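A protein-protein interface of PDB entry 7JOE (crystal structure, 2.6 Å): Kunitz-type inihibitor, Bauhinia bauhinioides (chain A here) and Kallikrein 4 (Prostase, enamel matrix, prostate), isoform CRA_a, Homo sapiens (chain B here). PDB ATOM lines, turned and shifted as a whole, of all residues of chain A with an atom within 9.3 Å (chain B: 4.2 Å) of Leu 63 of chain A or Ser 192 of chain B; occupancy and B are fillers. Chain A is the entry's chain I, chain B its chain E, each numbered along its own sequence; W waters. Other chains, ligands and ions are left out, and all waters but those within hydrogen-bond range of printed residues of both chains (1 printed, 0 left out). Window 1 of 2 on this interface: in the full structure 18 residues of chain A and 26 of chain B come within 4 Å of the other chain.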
ATOM      1  N   SER A  13      16.771 -19.407   0.398  1.00  0.00           N
ATOM      2  CA  SER A  13      16.922 -17.939   0.471  1.00  0.00           C
ATOM      3  C   SER A  13      15.708 -17.365   1.187  1.00  0.00           C
ATOM      4  O   SER A  13      14.682 -18.069   1.229  1.00  0.00           O
ATOM      5  CB  SER A  13      17.016 -17.397  -0.898  1.00  0.00           C
ATOM      6  OG  SER A  13      15.759 -17.507  -1.489  1.00  0.00           O
ATOM      7  N   ASN A  14      15.779 -16.113   1.611  1.00  0.00           N
ATOM      8  CA  ASN A  14      14.662 -15.458   2.320  1.00  0.00           C
ATOM      9  C   ASN A  14      13.930 -14.602   1.287  1.00  0.00           C
ATOM     10  O   ASN A  14      14.287 -13.464   1.124  1.00  0.00           O
ATOM     11  CB  ASN A  14      15.205 -14.710   3.539  1.00  0.00           C
ATOM     12  CG  ASN A  14      14.318 -13.597   4.059  1.00  0.00           C
ATOM     13  OD1 ASN A  14      13.214 -13.354   3.555  1.00  0.00           O
ATOM     14  ND2 ASN A  14      14.828 -12.882   5.049  1.00  0.00           N
ATOM     15  N   GLY A  15      12.934 -15.149   0.599  1.00  0.00           N
ATOM     16  CA  GLY A  15      12.046 -14.400  -0.320  1.00  0.00           C
ATOM     17  C   GLY A  15      12.657 -14.251  -1.701  1.00  0.00           C
ATOM     18  O   GLY A  15      11.897 -14.222  -2.689  1.00  0.00           O
ATOM     19  N   PHE A  59       9.488 -18.029   1.100  1.00  0.00           N
ATOM     20  CA  PHE A  59       9.560 -17.885   2.570  1.00  0.00           C
ATOM     21  C   PHE A  59      10.175 -16.544   2.935  1.00  0.00           C
ATOM     22  O   PHE A  59      11.321 -16.277   2.494  1.00  0.00           O
ATOM     23  CB  PHE A  59      10.451 -18.957   3.145  1.00  0.00           C
ATOM     24  CG  PHE A  59      10.139 -20.320   2.628  1.00  0.00           C
ATOM     25  CD1 PHE A  59       9.207 -21.112   3.276  1.00  0.00           C
ATOM     26  CD2 PHE A  59      10.831 -20.845   1.543  1.00  0.00           C
ATOM     27  CE1 PHE A  59       8.960 -22.401   2.825  1.00  0.00           C
ATOM     28  CE2 PHE A  59      10.587 -22.141   1.091  1.00  0.00           C
ATOM     29  CZ  PHE A  59       9.642 -22.926   1.738  1.00  0.00           C
ATOM     30  N   GLU A  60       9.488 -15.734   3.722  1.00  0.00           N
ATOM     31  CA  GLU A  60       9.985 -14.409   4.094  1.00  0.00           C
ATOM     32  C   GLU A  60      10.152 -14.335   5.585  1.00  0.00           C
ATOM     33  O   GLU A  60       9.160 -14.682   6.273  1.00  0.00           O
ATOM     34  CB  GLU A  60       8.935 -13.343   3.932  1.00  0.00           C
ATOM     35  CG  GLU A  60       8.919 -12.685   2.583  1.00  0.00           C
ATOM     36  CD  GLU A  60       7.873 -11.581   2.517  1.00  0.00           C
ATOM     37  OE1 GLU A  60       7.140 -11.344   3.583  1.00  0.00           O
ATOM     38  OE2 GLU A  60       7.783 -10.998   1.403  1.00  0.00           O
ATOM     39  N   SER A  61      11.307 -13.814   6.033  1.00  0.00           N
ATOM     40  CA  SER A  61      11.488 -13.172   7.360  1.00  0.00           C
ATOM     41  C   SER A  61      11.725 -11.688   7.158  1.00  0.00           C
ATOM     42  O   SER A  61      12.454 -11.297   6.251  1.00  0.00           O
ATOM     43  CB  SER A  61      12.634 -13.712   8.194  1.00  0.00           C
ATOM     44  OG  SER A  61      12.380 -13.396   9.582  1.00  0.00           O
ATOM     45  N   PRO A  62      11.271 -10.863   8.112  1.00  0.00           N
ATOM     46  CA  PRO A  62      11.694  -9.474   8.166  1.00  0.00           C
ATOM     47  C   PRO A  62      13.212  -9.287   8.414  1.00  0.00           C
ATOM     48  O   PRO A  62      13.721  -8.249   8.045  1.00  0.00           O
ATOM     49  CB  PRO A  62      10.853  -8.969   9.346  1.00  0.00           C
ATOM     50  CG  PRO A  62      10.686 -10.153  10.230  1.00  0.00           C
ATOM     51  CD  PRO A  62      10.448 -11.266   9.252  1.00  0.00           C
ATOM     52  N   LEU A  63      13.892 -10.269   9.028  1.00  0.00           N
ATOM     53  CA  LEU A  63      15.359 -10.208   9.354  1.00  0.00           C
ATOM     54  C   LEU A  63      16.119 -10.071   8.035  1.00  0.00           C
ATOM     55  O   LEU A  63      15.690 -10.700   7.019  1.00  0.00           O
ATOM     56  CB  LEU A  63      15.868 -11.476  10.061  1.00  0.00           C
ATOM     57  CG  LEU A  63      15.119 -11.965  11.306  1.00  0.00           C
ATOM     58  CD1 LEU A  63      15.605 -13.370  11.627  1.00  0.00           C
ATOM     59  CD2 LEU A  63      15.268 -11.035  12.511  1.00  0.00           C
ATOM     60  N   ARG A  64      17.195  -9.297   8.036  1.00  0.00           N
ATOM     61  CA  ARG A  64      17.842  -8.862   6.789  1.00  0.00           C
ATOM     62  C   ARG A  64      18.903  -9.878   6.425  1.00  0.00           C
ATOM     63  O   ARG A  64      19.989  -9.488   6.088  1.00  0.00           O
ATOM     64  CB  ARG A  64      18.379  -7.450   6.991  1.00  0.00           C
ATOM     65  CG  ARG A  64      17.254  -6.438   7.006  1.00  0.00           C
ATOM     66  CD  ARG A  64      16.569  -6.499   5.670  1.00  0.00           C
ATOM     67  NE  ARG A  64      15.792  -5.285   5.524  1.00  0.00           N
ATOM     68  CZ  ARG A  64      14.482  -5.249   5.362  1.00  0.00           C
ATOM     69  NH1 ARG A  64      13.826  -6.396   5.274  1.00  0.00           N
ATOM     70  NH2 ARG A  64      13.868  -4.069   5.261  1.00  0.00           N
ATOM     71  N   ILE A  65      18.545 -11.143   6.482  1.00  0.00           N
ATOM     72  CA  ILE A  65      19.446 -12.281   6.165  1.00  0.00           C
ATOM     73  C   ILE A  65      18.962 -12.846   4.836  1.00  0.00           C
ATOM     74  O   ILE A  65      17.892 -12.518   4.478  1.00  0.00           O
ATOM     75  CB  ILE A  65      19.487 -13.326   7.302  1.00  0.00           C
ATOM     76  CG1 ILE A  65      20.719 -14.226   7.196  1.00  0.00           C
ATOM     77  CG2 ILE A  65      18.194 -14.123   7.300  1.00  0.00           C
ATOM     78  CD1 ILE A  65      21.008 -15.053   8.403  1.00  0.00           C
ATOM     79  N   ASN A  66      19.848 -13.507   4.086  1.00  0.00           N
ATOM     80  CA  ASN A  66      19.587 -14.004   2.703  1.00  0.00           C
ATOM     81  C   ASN A  66      19.437 -15.530   2.785  1.00  0.00           C
ATOM     82  O   ASN A  66      19.396 -16.185   1.692  1.00  0.00           O
ATOM     83  CB  ASN A  66      20.607 -13.458   1.687  1.00  0.00           C
ATOM     84  CG  ASN A  66      22.028 -14.023   1.736  1.00  0.00           C
ATOM     85  OD1 ASN A  66      22.883 -13.553   0.974  1.00  0.00           O
ATOM     86  ND2 ASN A  66      22.323 -14.991   2.601  1.00  0.00           N
ATOM     87  N   ILE A  67      19.330 -16.040   4.030  1.00  0.00           N
ATOM     88  CA  ILE A  67      18.916 -17.438   4.305  1.00  0.00           C
ATOM     89  C   ILE A  67      17.848 -17.589   5.413  1.00  0.00           C
ATOM     90  O   ILE A  67      17.452 -16.625   6.059  1.00  0.00           O
ATOM     91  CB  ILE A  67      20.163 -18.275   4.573  1.00  0.00           C
ATOM     92  CG1 ILE A  67      20.925 -17.805   5.803  1.00  0.00           C
ATOM     93  CG2 ILE A  67      21.031 -18.303   3.340  1.00  0.00           C
ATOM     94  CD1 ILE A  67      22.030 -18.748   6.186  1.00  0.00           C
ATOM     95  N   ILE A  68      17.330 -18.812   5.530  1.00  0.00           N
ATOM     96  CA  ILE A  68      16.234 -19.249   6.433  1.00  0.00           C
ATOM     97  C   ILE A  68      16.796 -20.308   7.380  1.00  0.00           C
ATOM     98  O   ILE A  68      17.307 -21.350   6.885  1.00  0.00           O
ATOM     99  CB  ILE A  68      15.087 -19.841   5.582  1.00  0.00           C
ATOM    100  CG1 ILE A  68      14.386 -18.785   4.743  1.00  0.00           C
ATOM    101  CG2 ILE A  68      14.078 -20.588   6.431  1.00  0.00           C
ATOM    102  CD1 ILE A  68      13.942 -17.612   5.557  1.00  0.00           C
ATOM    103  N   LYS A  69      16.634 -20.070   8.673  1.00  0.00           N
ATOM    104  CA  LYS A  69      16.899 -21.037   9.769  1.00  0.00           C
ATOM    105  C   LYS A  69      15.588 -21.717  10.192  1.00  0.00           C
ATOM    106  O   LYS A  69      14.548 -21.069  10.232  1.00  0.00           O
ATOM    107  CB  LYS A  69      17.520 -20.310  10.975  1.00  0.00           C
ATOM    108  CG  LYS A  69      18.946 -19.780  10.785  1.00  0.00           C
ATOM    109  CD  LYS A  69      19.728 -19.655  12.079  1.00  0.00           C
ATOM    110  CE  LYS A  69      20.354 -18.294  12.300  1.00  0.00           C
ATOM    111  NZ  LYS A  69      20.883 -18.165  13.680  1.00  0.00           N
ATOM    112  N   SER A  71      14.410 -21.884  12.901  1.00  0.00           N
ATOM    113  CA  SER A  71      13.871 -21.275  14.147  1.00  0.00           C
ATOM    114  C   SER A  71      13.158 -19.955  13.853  1.00  0.00           C
ATOM    115  O   SER A  71      12.648 -19.350  14.802  1.00  0.00           O
ATOM    116  CB  SER A  71      14.950 -21.059  15.136  1.00  0.00           C
ATOM    117  OG  SER A  71      15.742 -19.930  14.772  1.00  0.00           O
ATOM    118  N   TYR A  72      13.193 -19.486  12.601  1.00  0.00           N
ATOM    119  CA  TYR A  72      12.586 -18.189  12.187  1.00  0.00           C
ATOM    120  C   TYR A  72      11.066 -18.395  12.010  1.00  0.00           C
ATOM    121  O   TYR A  72      10.701 -19.311  11.257  1.00  0.00           O
ATOM    122  CB  TYR A  72      13.170 -17.671  10.863  1.00  0.00           C
ATOM    123  CG  TYR A  72      14.623 -17.248  10.837  1.00  0.00           C
ATOM    124  CD1 TYR A  72      15.363 -16.994  11.992  1.00  0.00           C
ATOM    125  CD2 TYR A  72      15.261 -17.053   9.615  1.00  0.00           C
ATOM    126  CE1 TYR A  72      16.683 -16.578  11.925  1.00  0.00           C
ATOM    127  CE2 TYR A  72      16.573 -16.649   9.531  1.00  0.00           C
ATOM    128  CZ  TYR A  72      17.292 -16.400  10.688  1.00  0.00           C
ATOM    129  OH  TYR A  72      18.620 -16.017  10.584  1.00  0.00           O
ATOM    130  N   PHE A  73      10.220 -17.539  12.611  1.00  0.00           N
ATOM    131  CA  PHE A  73       8.832 -17.239  12.163  1.00  0.00           C
ATOM    132  C   PHE A  73       8.833 -16.747  10.721  1.00  0.00           C
ATOM    133  O   PHE A  73       9.591 -15.880  10.419  1.00  0.00           O
ATOM    134  CB  PHE A  73       8.201 -16.220  13.096  1.00  0.00           C
ATOM    135  CG  PHE A  73       7.795 -16.853  14.399  1.00  0.00           C
ATOM    136  CD1 PHE A  73       6.789 -17.822  14.435  1.00  0.00           C
ATOM    137  CD2 PHE A  73       8.430 -16.515  15.578  1.00  0.00           C
ATOM    138  CE1 PHE A  73       6.425 -18.424  15.630  1.00  0.00           C
ATOM    139  CE2 PHE A  73       8.075 -17.132  16.778  1.00  0.00           C
ATOM    140  CZ  PHE A  73       7.059 -18.080  16.809  1.00  0.00           C
ATOM    141  N   LEU A  74       8.037 -17.345   9.860  1.00  0.00           N
ATOM    142  CA  LEU A  74       8.002 -17.043   8.419  1.00  0.00           C
ATOM    143  C   LEU A  74       6.600 -16.638   8.007  1.00  0.00           C
ATOM    144  O   LEU A  74       5.640 -16.979   8.747  1.00  0.00           O
ATOM    145  CB  LEU A  74       8.412 -18.309   7.679  1.00  0.00           C
ATOM    146  CG  LEU A  74       9.829 -18.761   7.995  1.00  0.00           C
ATOM    147  CD1 LEU A  74      10.318 -19.743   6.974  1.00  0.00           C
ATOM    148  CD2 LEU A  74      10.747 -17.573   8.053  1.00  0.00           C
ATOM    149  N   LEU A 108       4.053  -8.617   9.994  1.00  0.00           N
ATOM    150  CA  LEU A 108       5.526  -8.473   9.840  1.00  0.00           C
ATOM    151  C   LEU A 108       6.233  -9.820  10.133  1.00  0.00           C
ATOM    152  O   LEU A 108       7.095 -10.220   9.316  1.00  0.00           O
ATOM    153  CB  LEU A 108       6.037  -7.353  10.749  1.00  0.00           C
ATOM    154  CG  LEU A 108       7.520  -7.064  10.604  1.00  0.00           C
ATOM    155  CD1 LEU A 108       7.742  -5.928   9.630  1.00  0.00           C
ATOM    156  CD2 LEU A 108       8.125  -6.749  11.956  1.00  0.00           C
ATOM    157  N   LEU A 109       5.823 -10.480  11.226  1.00  0.00           N
ATOM    158  CA  LEU A 109       6.205 -11.844  11.676  1.00  0.00           C
ATOM    159  C   LEU A 109       5.123 -12.890  11.295  1.00  0.00           C
ATOM    160  O   LEU A 109       4.192 -13.049  12.077  1.00  0.00           O
ATOM    161  CB  LEU A 109       6.336 -11.736  13.199  1.00  0.00           C
ATOM    162  CG  LEU A 109       7.600 -12.347  13.799  1.00  0.00           C
ATOM    163  CD1 LEU A 109       8.839 -11.839  13.082  1.00  0.00           C
ATOM    164  CD2 LEU A 109       7.673 -12.105  15.315  1.00  0.00           C
ATOM    165  N   HIS B  41      20.527 -13.121  15.454  1.00  0.00           N
ATOM    166  CA  HIS B  41      19.858 -13.941  14.415  1.00  0.00           C
ATOM    167  C   HIS B  41      20.862 -14.415  13.381  1.00  0.00           C
ATOM    168  O   HIS B  41      20.408 -15.126  12.500  1.00  0.00           O
ATOM    169  CB  HIS B  41      18.689 -13.172  13.775  1.00  0.00           C
ATOM    170  CG  HIS B  41      19.039 -12.192  12.679  1.00  0.00           C
ATOM    171  ND1 HIS B  41      18.966 -10.808  12.870  1.00  0.00           N
ATOM    172  CD2 HIS B  41      19.389 -12.392  11.375  1.00  0.00           C
ATOM    173  CE1 HIS B  41      19.395 -10.216  11.756  1.00  0.00           C
ATOM    174  NE2 HIS B  41      19.652 -11.173  10.811  1.00  0.00           N
ATOM    175  N   LEU B  83      12.171 -10.589  18.248  1.00  0.00           N
ATOM    176  CA  LEU B  83      13.050  -9.725  17.446  1.00  0.00           C
ATOM    177  C   LEU B  83      13.940  -8.820  18.311  1.00  0.00           C
ATOM    178  O   LEU B  83      14.821  -8.167  17.691  1.00  0.00           O
ATOM    179  CB  LEU B  83      12.170  -8.953  16.472  1.00  0.00           C
ATOM    180  CG  LEU B  83      11.396  -9.831  15.492  1.00  0.00           C
ATOM    181  CD1 LEU B  83      10.616  -8.965  14.528  1.00  0.00           C
ATOM    182  CD2 LEU B  83      12.282 -10.761  14.686  1.00  0.00           C
ATOM    183  N   ASP B  86      18.802  -8.139  19.591  1.00  0.00           N
ATOM    184  CA  ASP B  86      19.331  -8.918  18.437  1.00  0.00           C
ATOM    185  C   ASP B  86      20.857  -8.642  18.267  1.00  0.00           C
ATOM    186  O   ASP B  86      21.272  -7.984  17.236  1.00  0.00           O
ATOM    187  CB  ASP B  86      18.536  -8.600  17.167  1.00  0.00           C
ATOM    188  CG  ASP B  86      18.897  -9.445  15.950  1.00  0.00           C
ATOM    189  OD1 ASP B  86      19.514 -10.486  16.159  1.00  0.00           O
ATOM    190  OD2 ASP B  86      18.500  -9.094  14.789  1.00  0.00           O
ATOM    191  N   ASN B 174      18.620  -7.810   2.015  1.00  0.00           N
ATOM    192  CA  ASN B 174      18.907  -9.180   2.491  1.00  0.00           C
ATOM    193  C   ASN B 174      20.394  -9.483   2.294  1.00  0.00           C
ATOM    194  O   ASN B 174      20.864  -9.349   1.175  1.00  0.00           O
ATOM    195  CB  ASN B 174      17.986 -10.187   1.812  1.00  0.00           C
ATOM    196  CG  ASN B 174      16.583 -10.217   2.384  1.00  0.00           C
ATOM    197  OD1 ASN B 174      16.171  -9.377   3.176  1.00  0.00           O
ATOM    198  ND2 ASN B 174      15.843 -11.229   2.014  1.00  0.00           N
ATOM    199  N   SER B 177      22.416  -7.948   7.174  1.00  0.00           N
ATOM    200  CA  SER B 177      22.229  -8.235   8.620  1.00  0.00           C
ATOM    201  C   SER B 177      23.579  -8.204   9.370  1.00  0.00           C
ATOM    202  O   SER B 177      24.562  -8.883   8.925  1.00  0.00           O
ATOM    203  CB  SER B 177      21.526  -9.543   8.794  1.00  0.00           C
ATOM    204  OG  SER B 177      20.166  -9.355   9.150  1.00  0.00           O
ATOM    205  N   LEU B 190      23.424  -2.025  14.543  1.00  0.00           N
ATOM    206  CA  LEU B 190      23.514  -3.094  13.492  1.00  0.00           C
ATOM    207  C   LEU B 190      22.168  -3.286  12.730  1.00  0.00           C
ATOM    208  O   LEU B 190      21.067  -3.089  13.344  1.00  0.00           O
ATOM    209  CB  LEU B 190      23.931  -4.456  14.081  1.00  0.00           C
ATOM    210  CG  LEU B 190      24.948  -4.450  15.221  1.00  0.00           C
ATOM    211  CD1 LEU B 190      24.881  -5.728  16.037  1.00  0.00           C
ATOM    212  CD2 LEU B 190      26.329  -4.282  14.658  1.00  0.00           C
ATOM    213  N   VAL B 191      22.310  -3.747  11.466  1.00  0.00           N
ATOM    214  CA  VAL B 191      21.219  -4.105  10.547  1.00  0.00           C
ATOM    215  C   VAL B 191      20.539  -5.318  11.168  1.00  0.00           C
ATOM    216  O   VAL B 191      21.285  -6.260  11.539  1.00  0.00           O
ATOM    217  CB  VAL B 191      21.763  -4.359   9.131  1.00  0.00           C
ATOM    218  CG1 VAL B 191      20.709  -4.927   8.200  1.00  0.00           C
ATOM    219  CG2 VAL B 191      22.322  -3.104   8.499  1.00  0.00           C
ATOM    220  N   SER B 192      19.198  -5.254  11.321  1.00  0.00           N
ATOM    221  CA  SER B 192      18.338  -6.245  12.043  1.00  0.00           C
ATOM    222  C   SER B 192      17.181  -6.647  11.116  1.00  0.00           C
ATOM    223  O   SER B 192      17.286  -7.701  10.491  1.00  0.00           O
ATOM    224  CB  SER B 192      17.858  -5.681  13.392  1.00  0.00           C
ATOM    225  OG  SER B 192      17.092  -6.612  14.150  1.00  0.00           O
ATOM    226  N   PHE B 193      16.147  -5.823  10.954  1.00  0.00           N
ATOM    227  CA  PHE B 193      14.931  -6.224  10.202  1.00  0.00           C
ATOM    228  C   PHE B 193      14.255  -4.988   9.642  1.00  0.00           C
ATOM    229  O   PHE B 193      14.745  -3.893   9.793  1.00  0.00           O
ATOM    230  CB  PHE B 193      13.967  -7.082  11.046  1.00  0.00           C
ATOM    231  CG  PHE B 193      13.279  -6.397  12.212  1.00  0.00           C
ATOM    232  CD1 PHE B 193      13.910  -6.252  13.439  1.00  0.00           C
ATOM    233  CD2 PHE B 193      11.966  -5.949  12.116  1.00  0.00           C
ATOM    234  CE1 PHE B 193      13.251  -5.676  14.515  1.00  0.00           C
ATOM    235  CE2 PHE B 193      11.319  -5.360  13.192  1.00  0.00           C
ATOM    236  CZ  PHE B 193      11.946  -5.260  14.399  1.00  0.00           C
ATOM    237  N   VAL B 206      14.839  -1.353  10.906  1.00  0.00           N
ATOM    238  CA  VAL B 206      15.109  -1.421  12.375  1.00  0.00           C
ATOM    239  C   VAL B 206      16.567  -1.805  12.527  1.00  0.00           C
ATOM    240  O   VAL B 206      17.095  -2.523  11.643  1.00  0.00           O
ATOM    241  CB  VAL B 206      14.221  -2.442  13.101  1.00  0.00           C
ATOM    242  CG1 VAL B 206      14.253  -2.222  14.591  1.00  0.00           C
ATOM    243  CG2 VAL B 206      12.816  -2.406  12.576  1.00  0.00           C
ATOM    244  N   THR B 208      19.650  -2.788  15.735  1.00  0.00           N
ATOM    245  CA  THR B 208      19.916  -3.018  17.161  1.00  0.00           C
ATOM    246  C   THR B 208      20.533  -1.743  17.732  1.00  0.00           C
ATOM    247  O   THR B 208      21.557  -1.314  17.214  1.00  0.00           O
ATOM    248  CB  THR B 208      20.849  -4.201  17.431  1.00  0.00           C
ATOM    249  OG1 THR B 208      20.393  -5.371  16.744  1.00  0.00           O
ATOM    250  CG2 THR B 208      20.967  -4.468  18.920  1.00  0.00           C
HETATM  251  O   HOH W   1      17.387 -13.695   0.646  1.00  0.00           O
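ND2 of Asn 14 of chain A lies within hydrogen-bond range of O of Ser 61 of chain A (3.1 Å).
The side-chain amide nitrogen of Asn 14 of chain A sits at hydrogen-bond distance from the backbone carbonyl oxygen of Leu 63 of chain A (3.1 Å).
O of Pro 62 of chain A sits at hydrogen-bond distance from NH1 of Arg 64 of chain A (3.3 Å).
The backbone NH of Val 206 of chain B is in hydrogen-bond range of the backbone carbonyl oxygen of Phe 193 of chain B, 2.8 Å away.
ND1 of His 41 of chain B sits at hydrogen-bond distance from OD2 of Asp 86 of chain B, at 2.6 Å.
NE2 of His 41 of chain B lies within hydrogen-bond range of OG of Ser 177 of chain B, 2.5 Å away.
O of Pro 62 of chain A touches CA of Phe 193 of chain B (3.2 Å).
CD2 of Leu 63 of chain A touches ND1 of His 41 of chain B (3.7 Å).
Leu 83 of chain B touches Leu 63 of chain A (CD2 to CD2, 3.7 Å).
CB of Phe 193 of chain B touches N of Leu 63 of chain A, 3.8 Å away.
CA of Asn 174 of chain B touches O of Arg 64 of chain A (3.8 Å).
CG1 of Val 191 of chain B touches CB of Arg 64 of chain A (3.6 Å).
Arg 64 of chain A touches Phe 193 of chain B.
Ile 65 of chain A touches Ser 177 of chain B (N to OG, 3.6 Å).
Leu 108 of chain A touches Phe 193 of chain B.
Leu 109 of chain A touches Leu 83 of chain B (CD1 to CD1, 3.7 Å).
Leu 63 of chain A touches just these residues of chain B: His 41 (3.7 Å), Leu 83 (3.7 Å), Ser 192 (3.4 Å) and Phe 193 (3.8 Å).
Ser 192 of chain B touches just these residues of chain A: Leu 63 (3.4 Å) and Arg 64 (2.9 Å).
Val 191 of chain B touches just one residue of chain A: Arg 64.
Of the printed residues of chain B, Pro 62 of chain A touches Phe 193.
Printed residues of chain A within 4 Å of His 41 of chain B: Leu 63 (3.7 Å), Lys 69 (3.2 Å) and Tyr 72 (2.8 Å).
Of the printed residues of chain B, Arg 64 of chain A touches Asn 174 (3.8 Å), Ser 177 (3.0 Å), Val 191 (3.6 Å), Ser 192 (2.9 Å) and Phe 193 (3.96 Å).
Printed residues of chain B within 4 Å of Leu 108 of chain A: Phe 193 (3.7 Å).
The nearest printed residue of chain B that does not touch Ile 65 of chain A is His 41 of chain B (4.1 Å).
N of Arg 64 of chain A is in hydrogen-bond range of O of Ser 192 of chain B, at 2.9 Å.
O of His 41 of chain B lies within hydrogen-bond range of OH of Tyr 72 of chain A, at 2.8 Å.
OG of Ser 177 of chain B sits close to O of Arg 64 of chain A, 3.1 Å away.
The side-chain amide nitrogen (ND2) of Asn 174 of chain B sits at hydrogen-bond distance from the backbone carbonyl oxygen (O) of Asn 14 of chain A, at 2.9 Å.
The side-chain amino group (NZ) of Lys 69 of chain A sits close to the backbone carbonyl oxygen (O) of His 41 of chain B (3.3 Å).
O of Ile 65 of chain A sits close to ND2 of Asn 174 of chain B.
Water W1 lies within hydrogen-bond range of the backbone NH (N) of Asn 14 of chain A (3.1 Å), the side-chain amide nitrogen (ND2) of Asn 174 of chain B (3.2 Å) and the backbone carbonyl oxygen (O) of Asn 66 of chain A (3.4 Å).
Hydrophobic or aromatic side chains of chain A within 4 Å of the printed part of chain B: Leu 63, Tyr 72, Leu 108 and Leu 109.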
